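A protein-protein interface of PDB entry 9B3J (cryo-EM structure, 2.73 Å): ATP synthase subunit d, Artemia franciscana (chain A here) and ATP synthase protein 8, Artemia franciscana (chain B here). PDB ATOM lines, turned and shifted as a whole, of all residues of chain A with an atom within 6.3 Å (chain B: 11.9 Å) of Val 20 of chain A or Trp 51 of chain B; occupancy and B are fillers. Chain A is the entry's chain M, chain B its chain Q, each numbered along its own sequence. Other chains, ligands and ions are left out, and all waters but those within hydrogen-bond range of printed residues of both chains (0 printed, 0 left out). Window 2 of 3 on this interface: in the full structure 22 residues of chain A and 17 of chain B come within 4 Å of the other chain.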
ATOM      1  N   MET A  16      16.931 -28.096  22.976  1.00  0.00           N
ATOM      2  CA  MET A  16      18.142 -28.481  22.262  1.00  0.00           C
ATOM      3  C   MET A  16      18.830 -27.271  21.642  1.00  0.00           C
ATOM      4  O   MET A  16      20.063 -27.184  21.634  1.00  0.00           O
ATOM      5  CB  MET A  16      17.806 -29.512  21.190  1.00  0.00           C
ATOM      6  CG  MET A  16      19.021 -30.116  20.533  1.00  0.00           C
ATOM      7  SD  MET A  16      18.603 -31.419  19.374  1.00  0.00           S
ATOM      8  CE  MET A  16      20.231 -32.086  19.060  1.00  0.00           C
ATOM      9  N   ALA A  17      18.051 -26.324  21.128  1.00  0.00           N
ATOM     10  CA  ALA A  17      18.614 -25.174  20.437  1.00  0.00           C
ATOM     11  C   ALA A  17      19.139 -24.105  21.385  1.00  0.00           C
ATOM     12  O   ALA A  17      19.736 -23.130  20.918  1.00  0.00           O
ATOM     13  CB  ALA A  17      17.569 -24.562  19.503  1.00  0.00           C
ATOM     14  N   GLU A  18      18.938 -24.260  22.690  1.00  0.00           N
ATOM     15  CA  GLU A  18      19.360 -23.263  23.663  1.00  0.00           C
ATOM     16  C   GLU A  18      20.782 -23.478  24.160  1.00  0.00           C
ATOM     17  O   GLU A  18      21.225 -22.747  25.051  1.00  0.00           O
ATOM     18  CB  GLU A  18      18.401 -23.252  24.856  1.00  0.00           C
ATOM     19  CG  GLU A  18      16.985 -22.849  24.504  1.00  0.00           C
ATOM     20  CD  GLU A  18      16.071 -22.841  25.710  1.00  0.00           C
ATOM     21  OE1 GLU A  18      16.557 -23.122  26.824  1.00  0.00           O
ATOM     22  OE2 GLU A  18      14.866 -22.553  25.544  1.00  0.00           O
ATOM     23  N   SER A  19      21.505 -24.454  23.616  1.00  0.00           N
ATOM     24  CA  SER A  19      22.839 -24.753  24.114  1.00  0.00           C
ATOM     25  C   SER A  19      23.869 -24.800  22.995  1.00  0.00           C
ATOM     26  O   SER A  19      25.051 -24.524  23.223  1.00  0.00           O
ATOM     27  CB  SER A  19      22.838 -26.089  24.844  1.00  0.00           C
ATOM     28  OG  SER A  19      22.959 -27.136  23.899  1.00  0.00           O
ATOM     29  N   VAL A  20      23.431 -25.165  21.794  1.00  0.00           N
ATOM     30  CA  VAL A  20      24.331 -25.422  20.673  1.00  0.00           C
ATOM     31  C   VAL A  20      24.970 -24.118  20.199  1.00  0.00           C
ATOM     32  O   VAL A  20      24.263 -23.145  19.899  1.00  0.00           O
ATOM     33  CB  VAL A  20      23.592 -26.145  19.535  1.00  0.00           C
ATOM     34  CG1 VAL A  20      23.459 -27.619  19.864  1.00  0.00           C
ATOM     35  CG2 VAL A  20      22.210 -25.547  19.323  1.00  0.00           C
ATOM     36  N   PRO A  21      26.313 -24.044  20.143  1.00  0.00           N
ATOM     37  CA  PRO A  21      27.011 -22.815  19.746  1.00  0.00           C
ATOM     38  C   PRO A  21      27.154 -22.633  18.236  1.00  0.00           C
ATOM     39  O   PRO A  21      28.228 -22.289  17.735  1.00  0.00           O
ATOM     40  CB  PRO A  21      28.380 -22.970  20.420  1.00  0.00           C
ATOM     41  CG  PRO A  21      28.250 -24.144  21.361  1.00  0.00           C
ATOM     42  CD  PRO A  21      27.234 -25.021  20.736  1.00  0.00           C
ATOM     43  N   GLU A  22      26.055 -22.867  17.509  1.00  0.00           N
ATOM     44  CA  GLU A  22      25.928 -22.626  16.073  1.00  0.00           C
ATOM     45  C   GLU A  22      26.974 -23.369  15.251  1.00  0.00           C
ATOM     46  O   GLU A  22      26.783 -24.537  14.901  1.00  0.00           O
ATOM     47  CB  GLU A  22      25.991 -21.125  15.770  1.00  0.00           C
ATOM     48  CG  GLU A  22      24.711 -20.567  15.171  1.00  0.00           C
ATOM     49  CD  GLU A  22      24.417 -21.126  13.792  1.00  0.00           C
ATOM     50  OE1 GLU A  22      25.376 -21.408  13.042  1.00  0.00           O
ATOM     51  OE2 GLU A  22      23.225 -21.287  13.457  1.00  0.00           O
ATOM     52  N   SER A  23      28.077 -22.683  14.931  1.00  0.00           N
ATOM     53  CA  SER A  23      29.114 -23.269  14.088  1.00  0.00           C
ATOM     54  C   SER A  23      29.821 -24.430  14.774  1.00  0.00           C
ATOM     55  O   SER A  23      30.322 -25.334  14.094  1.00  0.00           O
ATOM     56  CB  SER A  23      30.130 -22.198  13.689  1.00  0.00           C
ATOM     57  OG  SER A  23      30.768 -21.649  14.828  1.00  0.00           O
ATOM     58  N   GLN A  24      29.890 -24.415  16.108  1.00  0.00           N
ATOM     59  CA  GLN A  24      30.459 -25.544  16.836  1.00  0.00           C
ATOM     60  C   GLN A  24      29.607 -26.796  16.664  1.00  0.00           C
ATOM     61  O   GLN A  24      30.138 -27.897  16.480  1.00  0.00           O
ATOM     62  CB  GLN A  24      30.608 -25.192  18.315  1.00  0.00           C
ATOM     63  CG  GLN A  24      31.121 -26.336  19.174  1.00  0.00           C
ATOM     64  CD  GLN A  24      31.228 -25.971  20.642  1.00  0.00           C
ATOM     65  OE1 GLN A  24      31.478 -24.817  20.991  1.00  0.00           O
ATOM     66  NE2 GLN A  24      31.038 -26.957  21.512  1.00  0.00           N
ATOM     67  N   LYS A  25      28.285 -26.643  16.702  1.00  0.00           N
ATOM     68  CA  LYS A  25      27.381 -27.780  16.602  1.00  0.00           C
ATOM     69  C   LYS A  25      26.448 -27.642  15.407  1.00  0.00           C
ATOM     70  O   LYS A  25      25.232 -27.820  15.538  1.00  0.00           O
ATOM     71  CB  LYS A  25      26.584 -27.939  17.898  1.00  0.00           C
ATOM     72  CG  LYS A  25      27.453 -28.277  19.101  1.00  0.00           C
ATOM     73  CD  LYS A  25      28.363 -29.452  18.793  1.00  0.00           C
ATOM     74  CE  LYS A  25      29.460 -29.618  19.825  1.00  0.00           C
ATOM     75  NZ  LYS A  25      30.487 -30.576  19.337  1.00  0.00           N
ATOM     76  N   TYR A  28      23.801 -30.259  14.344  1.00  0.00           N
ATOM     77  CA  TYR A  28      22.424 -30.209  14.823  1.00  0.00           C
ATOM     78  C   TYR A  28      21.471 -29.790  13.714  1.00  0.00           C
ATOM     79  O   TYR A  28      20.333 -30.276  13.658  1.00  0.00           O
ATOM     80  CB  TYR A  28      22.322 -29.259  16.016  1.00  0.00           C
ATOM     81  CG  TYR A  28      20.959 -28.635  16.204  1.00  0.00           C
ATOM     82  CD1 TYR A  28      19.903 -29.369  16.725  1.00  0.00           C
ATOM     83  CD2 TYR A  28      20.732 -27.307  15.871  1.00  0.00           C
ATOM     84  CE1 TYR A  28      18.657 -28.801  16.900  1.00  0.00           C
ATOM     85  CE2 TYR A  28      19.490 -26.731  16.041  1.00  0.00           C
ATOM     86  CZ  TYR A  28      18.458 -27.482  16.557  1.00  0.00           C
ATOM     87  OH  TYR A  28      17.219 -26.910  16.730  1.00  0.00           O
ATOM     88  N   GLU A 100      32.490 -38.595  30.051  1.00  0.00           N
ATOM     89  CA  GLU A 100      33.056 -37.332  29.589  1.00  0.00           C
ATOM     90  C   GLU A 100      32.352 -36.134  30.210  1.00  0.00           C
ATOM     91  O   GLU A 100      32.994 -35.115  30.484  1.00  0.00           O
ATOM     92  CB  GLU A 100      32.992 -37.250  28.065  1.00  0.00           C
ATOM     93  CG  GLU A 100      33.902 -38.235  27.356  1.00  0.00           C
ATOM     94  CD  GLU A 100      33.825 -38.112  25.849  1.00  0.00           C
ATOM     95  OE1 GLU A 100      33.089 -37.228  25.363  1.00  0.00           O
ATOM     96  OE2 GLU A 100      34.501 -38.898  25.152  1.00  0.00           O
ATOM     97  N   VAL B  47      35.850 -23.245  26.503  1.00  0.00           N
ATOM     98  CA  VAL B  47      35.313 -23.960  25.353  1.00  0.00           C
ATOM     99  C   VAL B  47      34.293 -24.965  25.866  1.00  0.00           C
ATOM    100  O   VAL B  47      34.572 -25.708  26.815  1.00  0.00           O
ATOM    101  CB  VAL B  47      36.423 -24.661  24.548  1.00  0.00           C
ATOM    102  CG1 VAL B  47      35.844 -25.357  23.328  1.00  0.00           C
ATOM    103  CG2 VAL B  47      37.492 -23.662  24.137  1.00  0.00           C
ATOM    104  N   TYR B  48      33.114 -24.975  25.253  1.00  0.00           N
ATOM    105  CA  TYR B  48      32.060 -25.883  25.666  1.00  0.00           C
ATOM    106  C   TYR B  48      32.426 -27.324  25.325  1.00  0.00           C
ATOM    107  O   TYR B  48      33.292 -27.596  24.488  1.00  0.00           O
ATOM    108  CB  TYR B  48      30.739 -25.515  24.993  1.00  0.00           C
ATOM    109  CG  TYR B  48      30.430 -24.037  24.997  1.00  0.00           C
ATOM    110  CD1 TYR B  48      29.847 -23.432  26.103  1.00  0.00           C
ATOM    111  CD2 TYR B  48      30.707 -23.247  23.886  1.00  0.00           C
ATOM    112  CE1 TYR B  48      29.557 -22.081  26.106  1.00  0.00           C
ATOM    113  CE2 TYR B  48      30.421 -21.896  23.880  1.00  0.00           C
ATOM    114  CZ  TYR B  48      29.846 -21.320  24.992  1.00  0.00           C
ATOM    115  OH  TYR B  48      29.561 -19.974  24.986  1.00  0.00           O
ATOM    116  N   LEU B  49      31.752 -28.255  25.995  1.00  0.00           N
ATOM    117  CA  LEU B  49      32.004 -29.671  25.771  1.00  0.00           C
ATOM    118  C   LEU B  49      31.468 -30.099  24.411  1.00  0.00           C
ATOM    119  O   LEU B  49      30.314 -29.824  24.070  1.00  0.00           O
ATOM    120  CB  LEU B  49      31.361 -30.504  26.878  1.00  0.00           C
ATOM    121  CG  LEU B  49      31.409 -32.023  26.705  1.00  0.00           C
ATOM    122  CD1 LEU B  49      32.842 -32.511  26.563  1.00  0.00           C
ATOM    123  CD2 LEU B  49      30.726 -32.702  27.876  1.00  0.00           C
ATOM    124  N   ASN B  50      32.309 -30.780  23.641  1.00  0.00           N
ATOM    125  CA  ASN B  50      31.907 -31.265  22.330  1.00  0.00           C
ATOM    126  C   ASN B  50      31.017 -32.491  22.469  1.00  0.00           C
ATOM    127  O   ASN B  50      31.262 -33.365  23.303  1.00  0.00           O
ATOM    128  CB  ASN B  50      33.132 -31.599  21.483  1.00  0.00           C
ATOM    129  CG  ASN B  50      34.012 -30.394  21.239  1.00  0.00           C
ATOM    130  OD1 ASN B  50      33.552 -29.254  21.309  1.00  0.00           O
ATOM    131  ND2 ASN B  50      35.283 -30.637  20.950  1.00  0.00           N
ATOM    132  N   TRP B  51      29.981 -32.547  21.643  1.00  0.00           N
ATOM    133  CA  TRP B  51      29.028 -33.643  21.676  1.00  0.00           C
ATOM    134  C   TRP B  51      29.522 -34.754  20.756  1.00  0.00           C
ATOM    135  O   TRP B  51      30.667 -34.749  20.296  1.00  0.00           O
ATOM    136  CB  TRP B  51      27.635 -33.166  21.270  1.00  0.00           C
ATOM    137  CG  TRP B  51      27.015 -32.133  22.168  1.00  0.00           C
ATOM    138  CD1 TRP B  51      27.593 -31.496  23.230  1.00  0.00           C
ATOM    139  CD2 TRP B  51      25.682 -31.622  22.077  1.00  0.00           C
ATOM    140  NE1 TRP B  51      26.704 -30.619  23.798  1.00  0.00           N
ATOM    141  CE2 TRP B  51      25.522 -30.679  23.108  1.00  0.00           C
ATOM    142  CE3 TRP B  51      24.607 -31.870  21.220  1.00  0.00           C
ATOM    143  CZ2 TRP B  51      24.332 -29.985  23.303  1.00  0.00           C
ATOM    144  CZ3 TRP B  51      23.429 -31.183  21.416  1.00  0.00           C
ATOM    145  CH2 TRP B  51      23.300 -30.251  22.448  1.00  0.00           C
ATOM    146  N   LYS B  52      28.658 -35.723  20.475  1.00  0.00           N
ATOM    147  CA  LYS B  52      28.964 -36.790  19.536  1.00  0.00           C
ATOM    148  C   LYS B  52      27.976 -36.733  18.381  1.00  0.00           C
ATOM    149  O   LYS B  52      26.760 -36.725  18.596  1.00  0.00           O
ATOM    150  CB  LYS B  52      28.924 -38.157  20.220  1.00  0.00           C
ATOM    151  CG  LYS B  52      30.014 -38.342  21.266  1.00  0.00           C
ATOM    152  CD  LYS B  52      30.112 -39.790  21.713  1.00  0.00           C
ATOM    153  CE  LYS B  52      31.309 -40.010  22.624  1.00  0.00           C
ATOM    154  NZ  LYS B  52      31.481 -41.452  22.955  1.00  0.00           N
ATOM    155  N   TRP B  53      28.505 -36.678  17.165  1.00  0.00           N
ATOM    156  CA  TRP B  53      27.694 -36.639  15.958  1.00  0.00           C
ATOM    157  C   TRP B  53      28.158 -37.745  15.044  1.00  0.00           C
ATOM    158  O   TRP B  53      27.790 -37.855  13.873  1.00  0.00           O
ATOM    159  CB  TRP B  53      27.818 -35.292  15.263  1.00  0.00           C
ATOM    160  CG  TRP B  53      27.510 -34.168  16.163  1.00  0.00           C
ATOM    161  CD1 TRP B  53      28.397 -33.440  16.893  1.00  0.00           C
ATOM    162  CD2 TRP B  53      26.217 -33.641  16.455  1.00  0.00           C
ATOM    163  NE1 TRP B  53      27.736 -32.481  17.616  1.00  0.00           N
ATOM    164  CE2 TRP B  53      26.393 -32.583  17.363  1.00  0.00           C
ATOM    165  CE3 TRP B  53      24.924 -33.955  16.029  1.00  0.00           C
ATOM    166  CZ2 TRP B  53      25.330 -31.838  17.853  1.00  0.00           C
ATOM    167  CZ3 TRP B  53      23.868 -33.216  16.517  1.00  0.00           C
ATOM    168  CH2 TRP B  53      24.077 -32.171  17.421  1.00  0.00           C
ATOM    169  OXT TRP B  53      28.961 -38.536  15.513  1.00  0.00           O
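The side-chain amide oxygen of Asn 50 of chain B is in hydrogen-bond range of the side-chain amide nitrogen of Gln 24 of chain A, 3.4 Å away. The backbone NH of Trp 51 of chain B lies close to the side-chain amino group of Lys 25 of chain A (3.1 Å).
No residue of chain B comes within 4 Å of Met 16 of chain A. No residue of chain B comes within 4 Å of Ala 17 of chain A. Ser 19 of chain A touches just one residue of chain B: Trp 51. Glu 22 of chain A touches none of the printed residues of chain B. Gln 24 of chain A touches just these residues of chain B: Tyr 48 (3.4 Å), Leu 49 (3.9 Å) and Asn 50 (3.4 Å). Lys 25 of chain A touches just these residues of chain B: Asn 50, Trp 51 and Trp 53. Tyr 28 of chain A touches just one residue of chain B: Trp 53. Printed residues of chain A within 4 Å of Leu 49 of chain B: Gln 24 (3.9 Å). Of the printed residues of chain A, Trp 51 of chain B touches Ser 19 (3.2 Å), Val 20 (3.7 Å) and Lys 25 (3.1 Å). Lys 52 of chain B touches none of the printed residues of chain A. Printed residues of chain A within 4 Å of Trp 53 of chain B: Lys 25 (3.3 Å) and Tyr 28 (3.6 Å). The nearest residue of chain B that does not touch Val 20 of chain A is Trp 53 of chain B (5.0 Å). The nearest residue of chain A that does not touch Trp 51 of chain B is Met 16 of chain A (4.1 Å). The nearest printed residue of chain A that does not touch Tyr 48 of chain B is Ser 19 of chain A (5.7 Å).
Hydrophobic or aromatic side chains of chain A within 4 Å of the printed part of chain B: Val 20, Pro 21 and Tyr 28. Hydrophobic or aromatic side chains of chain B within 4 Å of the printed part of chain A: Tyr 48, Trp 51 and Trp 53. Along chain B the printed residues that touch a printed residue of chain A span positions 48 to 53. Among the printed residues, no Asp or Glu carboxylate lies within 4 Å of a Lys or Arg side-chain nitrogen of the other chain.
Among the printed residues, pairs that only touch across the chains: Ser 19 of chain A with Trp 51 of chain B (3.2 Å), Val 20 of chain A with Trp 51 of chain B (3.7 Å), Pro 21 of chain A with Tyr 48 of chain B (3.6 Å), Gln 24 of chain A with Tyr 48 of chain B (3.4 Å), Gln 24 of chain A with Leu 49 of chain B (3.9 Å), Lys 25 of chain A with Asn 50 of chain B (3.4 Å), Lys 25 of chain A with Trp 53 of chain B (3.3 Å) and Tyr 28 of chain A with Trp 53 of chain B (3.6 Å).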
